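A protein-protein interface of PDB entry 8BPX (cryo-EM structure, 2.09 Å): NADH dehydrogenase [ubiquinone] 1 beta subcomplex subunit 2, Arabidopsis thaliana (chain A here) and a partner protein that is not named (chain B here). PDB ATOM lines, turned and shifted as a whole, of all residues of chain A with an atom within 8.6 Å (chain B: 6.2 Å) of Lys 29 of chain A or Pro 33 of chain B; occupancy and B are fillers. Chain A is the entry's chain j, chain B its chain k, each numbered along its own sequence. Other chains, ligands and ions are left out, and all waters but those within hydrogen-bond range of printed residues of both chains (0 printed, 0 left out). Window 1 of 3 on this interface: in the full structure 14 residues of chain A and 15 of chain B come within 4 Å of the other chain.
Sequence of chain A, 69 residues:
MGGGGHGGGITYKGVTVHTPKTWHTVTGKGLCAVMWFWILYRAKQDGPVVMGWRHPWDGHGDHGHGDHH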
ATOM      1  N   THR A  22       5.705  -7.618  22.426  1.00  0.00           N
ATOM      2  CA  THR A  22       5.289  -6.573  23.355  1.00  0.00           C
ATOM      3  C   THR A  22       3.874  -6.088  23.062  1.00  0.00           C
ATOM      4  O   THR A  22       3.068  -5.922  23.984  1.00  0.00           O
ATOM      5  CB  THR A  22       6.289  -5.412  23.326  1.00  0.00           C
ATOM      6  OG1 THR A  22       5.826  -4.353  24.174  1.00  0.00           O
ATOM      7  CG2 THR A  22       6.502  -4.893  21.912  1.00  0.00           C
ATOM      8  N   TRP A  23       3.553  -5.907  21.776  1.00  0.00           N
ATOM      9  CA  TRP A  23       2.213  -5.381  21.400  1.00  0.00           C
ATOM     10  C   TRP A  23       1.139  -6.423  21.729  1.00  0.00           C
ATOM     11  O   TRP A  23      -0.005  -6.011  21.970  1.00  0.00           O
ATOM     12  CB  TRP A  23       2.185  -4.936  19.930  1.00  0.00           C
ATOM     13  CG  TRP A  23       1.981  -6.030  18.927  1.00  0.00           C
ATOM     14  CD1 TRP A  23       2.914  -6.912  18.464  1.00  0.00           C
ATOM     15  CD2 TRP A  23       0.760  -6.335  18.232  1.00  0.00           C
ATOM     16  NE1 TRP A  23       2.354  -7.753  17.540  1.00  0.00           N
ATOM     17  CE2 TRP A  23       1.036  -7.421  17.374  1.00  0.00           C
ATOM     18  CE3 TRP A  23      -0.533  -5.804  18.253  1.00  0.00           C
ATOM     19  CZ2 TRP A  23       0.060  -7.982  16.552  1.00  0.00           C
ATOM     20  CZ3 TRP A  23      -1.496  -6.360  17.440  1.00  0.00           C
ATOM     21  CH2 TRP A  23      -1.201  -7.436  16.602  1.00  0.00           C
ATOM     22  N   HIS A  24       1.492  -7.713  21.749  1.00  0.00           N
ATOM     23  CA  HIS A  24       0.534  -8.738  22.143  1.00  0.00           C
ATOM     24  C   HIS A  24       0.181  -8.616  23.621  1.00  0.00           C
ATOM     25  O   HIS A  24      -1.004  -8.609  23.994  1.00  0.00           O
ATOM     26  CB  HIS A  24       1.106 -10.117  21.826  1.00  0.00           C
ATOM     27  CG  HIS A  24       0.840 -10.561  20.423  1.00  0.00           C
ATOM     28  ND1 HIS A  24       1.173 -11.812  19.960  1.00  0.00           N
ATOM     29  CD2 HIS A  24       0.269  -9.915  19.381  1.00  0.00           C
ATOM     30  CE1 HIS A  24       0.820 -11.920  18.693  1.00  0.00           C
ATOM     31  NE2 HIS A  24       0.269 -10.781  18.316  1.00  0.00           N
ATOM     32  N   THR A  25       1.200  -8.496  24.474  1.00  0.00           N
ATOM     33  CA  THR A  25       0.959  -8.267  25.892  1.00  0.00           C
ATOM     34  C   THR A  25       0.151  -6.995  26.102  1.00  0.00           C
ATOM     35  O   THR A  25      -0.820  -6.988  26.865  1.00  0.00           O
ATOM     36  CB  THR A  25       2.283  -8.185  26.655  1.00  0.00           C
ATOM     37  OG1 THR A  25       3.020  -9.400  26.482  1.00  0.00           O
ATOM     38  CG2 THR A  25       2.031  -7.963  28.128  1.00  0.00           C
ATOM     39  N   VAL A  26       0.524  -5.917  25.409  1.00  0.00           N
ATOM     40  CA  VAL A  26      -0.146  -4.634  25.604  1.00  0.00           C
ATOM     41  C   VAL A  26      -1.606  -4.718  25.176  1.00  0.00           C
ATOM     42  O   VAL A  26      -2.501  -4.236  25.877  1.00  0.00           O
ATOM     43  CB  VAL A  26       0.603  -3.516  24.856  1.00  0.00           C
ATOM     44  CG1 VAL A  26      -0.246  -2.255  24.794  1.00  0.00           C
ATOM     45  CG2 VAL A  26       1.929  -3.230  25.535  1.00  0.00           C
ATOM     46  N   THR A  27      -1.867  -5.330  24.018  1.00  0.00           N
ATOM     47  CA  THR A  27      -3.234  -5.441  23.526  1.00  0.00           C
ATOM     48  C   THR A  27      -4.097  -6.273  24.467  1.00  0.00           C
ATOM     49  O   THR A  27      -5.244  -5.904  24.755  1.00  0.00           O
ATOM     50  CB  THR A  27      -3.227  -6.037  22.118  1.00  0.00           C
ATOM     51  OG1 THR A  27      -2.576  -5.132  21.219  1.00  0.00           O
ATOM     52  CG2 THR A  27      -4.630  -6.286  21.630  1.00  0.00           C
ATOM     53  N   GLY A  28      -3.568  -7.396  24.963  1.00  0.00           N
ATOM     54  CA  GLY A  28      -4.331  -8.192  25.912  1.00  0.00           C
ATOM     55  C   GLY A  28      -4.619  -7.444  27.199  1.00  0.00           C
ATOM     56  O   GLY A  28      -5.768  -7.384  27.660  1.00  0.00           O
ATOM     57  N   LYS A  29      -3.562  -6.938  27.868  1.00  0.00           N
ATOM     58  CA  LYS A  29      -3.820  -6.062  29.041  1.00  0.00           C
ATOM     59  C   LYS A  29      -4.883  -4.995  28.711  1.00  0.00           C
ATOM     60  O   LYS A  29      -5.862  -5.048  29.414  1.00  0.00           O
ATOM     61  CB  LYS A  29      -2.542  -5.453  29.625  1.00  0.00           C
ATOM     62  CG  LYS A  29      -1.676  -6.395  30.444  1.00  0.00           C
ATOM     63  CD  LYS A  29      -2.055  -6.409  31.899  1.00  0.00           C
ATOM     64  CE  LYS A  29      -1.295  -7.429  32.717  1.00  0.00           C
ATOM     65  NZ  LYS A  29      -1.454  -8.796  32.171  1.00  0.00           N
ATOM     66  N   GLY A  30      -4.758  -4.206  27.634  1.00  0.00           N
ATOM     67  CA  GLY A  30      -5.654  -3.084  27.434  1.00  0.00           C
ATOM     68  C   GLY A  30      -7.084  -3.488  27.157  1.00  0.00           C
ATOM     69  O   GLY A  30      -8.015  -2.869  27.675  1.00  0.00           O
ATOM     70  N   LEU A  31      -7.289  -4.514  26.326  1.00  0.00           N
ATOM     71  CA  LEU A  31      -8.651  -4.968  26.080  1.00  0.00           C
ATOM     72  C   LEU A  31      -9.294  -5.501  27.350  1.00  0.00           C
ATOM     73  O   LEU A  31     -10.464  -5.205  27.625  1.00  0.00           O
ATOM     74  CB  LEU A  31      -8.688  -6.018  24.974  1.00  0.00           C
ATOM     75  CG  LEU A  31      -8.795  -5.445  23.566  1.00  0.00           C
ATOM     76  CD1 LEU A  31      -8.006  -6.270  22.584  1.00  0.00           C
ATOM     77  CD2 LEU A  31     -10.253  -5.385  23.150  1.00  0.00           C
ATOM     78  N   CYS A  32      -8.579  -6.283  28.134  1.00  0.00           N
ATOM     79  CA  CYS A  32      -9.190  -6.699  29.401  1.00  0.00           C
ATOM     80  C   CYS A  32      -9.448  -5.488  30.324  1.00  0.00           C
ATOM     81  O   CYS A  32     -10.467  -5.531  30.995  1.00  0.00           O
ATOM     82  CB  CYS A  32      -8.392  -7.831  30.057  1.00  0.00           C
ATOM     83  SG  CYS A  32      -8.749  -9.448  29.314  1.00  0.00           S
ATOM     84  N   ALA A  33      -8.603  -4.466  30.308  1.00  0.00           N
ATOM     85  CA  ALA A  33      -8.769  -3.305  31.226  1.00  0.00           C
ATOM     86  C   ALA A  33     -10.030  -2.587  30.794  1.00  0.00           C
ATOM     87  O   ALA A  33     -10.874  -2.332  31.665  1.00  0.00           O
ATOM     88  CB  ALA A  33      -7.540  -2.418  31.237  1.00  0.00           C
ATOM     89  N   VAL A  34     -10.202  -2.506  29.484  1.00  0.00           N
ATOM     90  CA  VAL A  34     -11.404  -1.889  28.939  1.00  0.00           C
ATOM     91  C   VAL A  34     -12.635  -2.675  29.361  1.00  0.00           C
ATOM     92  O   VAL A  34     -13.661  -2.096  29.730  1.00  0.00           O
ATOM     93  CB  VAL A  34     -11.297  -1.776  27.405  1.00  0.00           C
ATOM     94  CG1 VAL A  34     -12.670  -1.746  26.760  1.00  0.00           C
ATOM     95  CG2 VAL A  34     -10.514  -0.546  27.018  1.00  0.00           C
ATOM     96  N   MET A  35     -12.549  -4.009  29.324  1.00  0.00           N
ATOM     97  CA  MET A  35     -13.677  -4.838  29.742  1.00  0.00           C
ATOM     98  C   MET A  35     -14.017  -4.624  31.216  1.00  0.00           C
ATOM     99  O   MET A  35     -15.193  -4.489  31.576  1.00  0.00           O
ATOM    100  CB  MET A  35     -13.367  -6.308  29.467  1.00  0.00           C
ATOM    101  CG  MET A  35     -14.226  -7.294  30.238  1.00  0.00           C
ATOM    102  SD  MET A  35     -13.760  -9.012  29.952  1.00  0.00           S
ATOM    103  CE  MET A  35     -12.160  -9.068  30.758  1.00  0.00           C
ATOM    104  N   TRP A  36     -13.044  -4.594  32.092  1.00  0.00           N
ATOM    105  CA  TRP A  36     -13.236  -4.379  33.561  1.00  0.00           C
ATOM    106  C   TRP A  36     -13.831  -2.988  33.817  1.00  0.00           C
ATOM    107  O   TRP A  36     -14.794  -2.918  34.572  1.00  0.00           O
ATOM    108  CB  TRP A  36     -11.948  -4.612  34.355  1.00  0.00           C
ATOM    109  CG  TRP A  36     -11.322  -5.962  34.202  1.00  0.00           C
ATOM    110  CD1 TRP A  36     -10.053  -6.233  33.787  1.00  0.00           C
ATOM    111  CD2 TRP A  36     -11.931  -7.234  34.476  1.00  0.00           C
ATOM    112  NE1 TRP A  36      -9.832  -7.578  33.771  1.00  0.00           N
ATOM    113  CE2 TRP A  36     -10.964  -8.221  34.192  1.00  0.00           C
ATOM    114  CE3 TRP A  36     -13.188  -7.640  34.924  1.00  0.00           C
ATOM    115  CZ2 TRP A  36     -11.221  -9.580  34.360  1.00  0.00           C
ATOM    116  CZ3 TRP A  36     -13.450  -8.983  35.076  1.00  0.00           C
ATOM    117  CH2 TRP A  36     -12.472  -9.942  34.797  1.00  0.00           C
ATOM    118  N   HIS B  30      -1.769 -14.268  36.793  1.00  0.00           N
ATOM    119  CA  HIS B  30      -1.972 -13.643  35.465  1.00  0.00           C
ATOM    120  C   HIS B  30      -3.389 -13.816  34.966  1.00  0.00           C
ATOM    121  O   HIS B  30      -3.625 -13.482  33.827  1.00  0.00           O
ATOM    122  CB  HIS B  30      -1.031 -14.331  34.489  1.00  0.00           C
ATOM    123  CG  HIS B  30       0.342 -13.770  34.529  1.00  0.00           C
ATOM    124  ND1 HIS B  30       1.272 -14.169  35.459  1.00  0.00           N
ATOM    125  CD2 HIS B  30       0.924 -12.808  33.788  1.00  0.00           C
ATOM    126  CE1 HIS B  30       2.382 -13.503  35.268  1.00  0.00           C
ATOM    127  NE2 HIS B  30       2.200 -12.665  34.249  1.00  0.00           N
ATOM    128  N   ALA B  31      -4.278 -14.337  35.779  1.00  0.00           N
ATOM    129  CA  ALA B  31      -5.632 -14.723  35.368  1.00  0.00           C
ATOM    130  C   ALA B  31      -6.575 -13.539  35.067  1.00  0.00           C
ATOM    131  O   ALA B  31      -7.502 -13.748  34.371  1.00  0.00           O
ATOM    132  CB  ALA B  31      -6.123 -15.588  36.470  1.00  0.00           C
ATOM    133  N   LEU B  32      -6.349 -12.366  35.677  1.00  0.00           N
ATOM    134  CA  LEU B  32      -7.226 -11.197  35.518  1.00  0.00           C
ATOM    135  C   LEU B  32      -6.379 -10.031  35.021  1.00  0.00           C
ATOM    136  O   LEU B  32      -6.174  -9.101  35.761  1.00  0.00           O
ATOM    137  CB  LEU B  32      -7.937 -10.984  36.867  1.00  0.00           C
ATOM    138  CG  LEU B  32      -8.812 -12.112  37.390  1.00  0.00           C
ATOM    139  CD1 LEU B  32      -9.234 -11.805  38.816  1.00  0.00           C
ATOM    140  CD2 LEU B  32     -10.017 -12.336  36.495  1.00  0.00           C
ATOM    141  N   PRO B  33      -5.905 -10.050  33.758  1.00  0.00           N
ATOM    142  CA  PRO B  33      -5.026  -9.040  33.217  1.00  0.00           C
ATOM    143  C   PRO B  33      -5.776  -7.727  33.039  1.00  0.00           C
ATOM    144  O   PRO B  33      -6.910  -7.749  32.719  1.00  0.00           O
ATOM    145  CB  PRO B  33      -4.614  -9.544  31.813  1.00  0.00           C
ATOM    146  CG  PRO B  33      -5.650 -10.567  31.426  1.00  0.00           C
ATOM    147  CD  PRO B  33      -6.250 -11.050  32.724  1.00  0.00           C
ATOM    148  N   GLY B  34      -5.056  -6.624  33.267  1.00  0.00           N
ATOM    149  CA  GLY B  34      -5.750  -5.323  33.297  1.00  0.00           C
ATOM    150  C   GLY B  34      -6.678  -5.125  34.488  1.00  0.00           C
ATOM    151  O   GLY B  34      -7.405  -4.163  34.437  1.00  0.00           O
ATOM    152  N   ILE B  35      -6.725  -5.970  35.488  1.00  0.00           N
ATOM    153  CA  ILE B  35      -7.692  -5.723  36.600  1.00  0.00           C
ATOM    154  C   ILE B  35      -7.227  -4.453  37.309  1.00  0.00           C
ATOM    155  O   ILE B  35      -8.062  -3.720  37.721  1.00  0.00           O
ATOM    156  CB  ILE B  35      -7.851  -6.869  37.603  1.00  0.00           C
ATOM    157  CG1 ILE B  35      -9.072  -6.712  38.513  1.00  0.00           C
ATOM    158  CG2 ILE B  35      -6.586  -7.069  38.421  1.00  0.00           C
ATOM    159  CD1 ILE B  35     -10.398  -6.973  37.846  1.00  0.00           C
ATOM    160  N   GLY B  36      -5.928  -4.196  37.295  1.00  0.00           N
ATOM    161  CA  GLY B  36      -5.415  -3.009  37.947  1.00  0.00           C
ATOM    162  C   GLY B  36      -5.675  -1.734  37.175  1.00  0.00           C
ATOM    163  O   GLY B  36      -6.166  -0.751  37.739  1.00  0.00           O
ATOM    164  N   ILE B  37      -5.345  -1.740  35.881  1.00  0.00           N
ATOM    165  CA  ILE B  37      -5.535  -0.555  35.049  1.00  0.00           C
ATOM    166  C   ILE B  37      -7.006  -0.187  34.965  1.00  0.00           C
ATOM    167  O   ILE B  37      -7.370   0.992  35.033  1.00  0.00           O
ATOM    168  CB  ILE B  37      -4.940  -0.780  33.648  1.00  0.00           C
ATOM    169  CG1 ILE B  37      -3.529  -1.352  33.748  1.00  0.00           C
ATOM    170  CG2 ILE B  37      -4.951   0.517  32.860  1.00  0.00           C
ATOM    171  CD1 ILE B  37      -3.290  -2.520  32.835  1.00  0.00           C
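The indole nitrogen of Trp 36 of chain A is in hydrogen-bond range of the backbone carbonyl oxygen of Pro 33 of chain B (3.1 Å).
Pro 33 of chain B touches Lys 29 of chain A (CB to NZ, 3.3 Å).
Lys 29 of chain A touches Gly 34 of chain B.
Pro 33 of chain B touches Cys 32 of chain A.
Ala 33 of chain A touches Gly 34 of chain B (CA to O, 3.6 Å).
CB of Ala 33 of chain A touches CB of Ile 37 of chain B, 3.9 Å away.
Trp 36 of chain A touches Leu 32 of chain B (CZ2 to CD2, 3.7 Å).
Gly 34 of chain B touches Trp 36 of chain A (O to CD1, 3.4 Å).
CA of Ile 35 of chain B touches CD1 of Trp 36 of chain A (3.7 Å).
Gly 28 of chain A touches none of the printed residues of chain B.
Of chain B, only Pro 33 and Gly 34 come within 4 Å of Lys 29 of chain A.
Of the printed residues of chain B, Cys 32 of chain A touches Pro 33 (3.0 Å).
Printed residues of chain B within 4 Å of Trp 36 of chain A: Leu 32 (3.7 Å), Pro 33 (3.1 Å), Gly 34 (3.4 Å) and Ile 35 (3.7 Å).
Pro 33 of chain B touches just these residues of chain A: Lys 29, Cys 32 and Trp 36.
Printed residues of chain A within 4 Å of Ile 37 of chain B: Ala 33.
The nearest residue of chain B that does not touch Lys 29 of chain A is Ile 37 of chain B (4.2 Å).
The nearest residue of chain A that does not touch Pro 33 of chain B is Ala 33 of chain A (4.4 Å).
The nearest printed residue of chain A that does not touch Ile 35 of chain B is Ala 33 of chain A (5.4 Å).
Hydrophobic or aromatic side chains of chain A within 4 Å of the printed part of chain B: Ala 33 and Trp 36.
Among the printed residues, no Asp or Glu carboxylate lies within 4 Å of a Lys or Arg side-chain nitrogen of the other chain.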
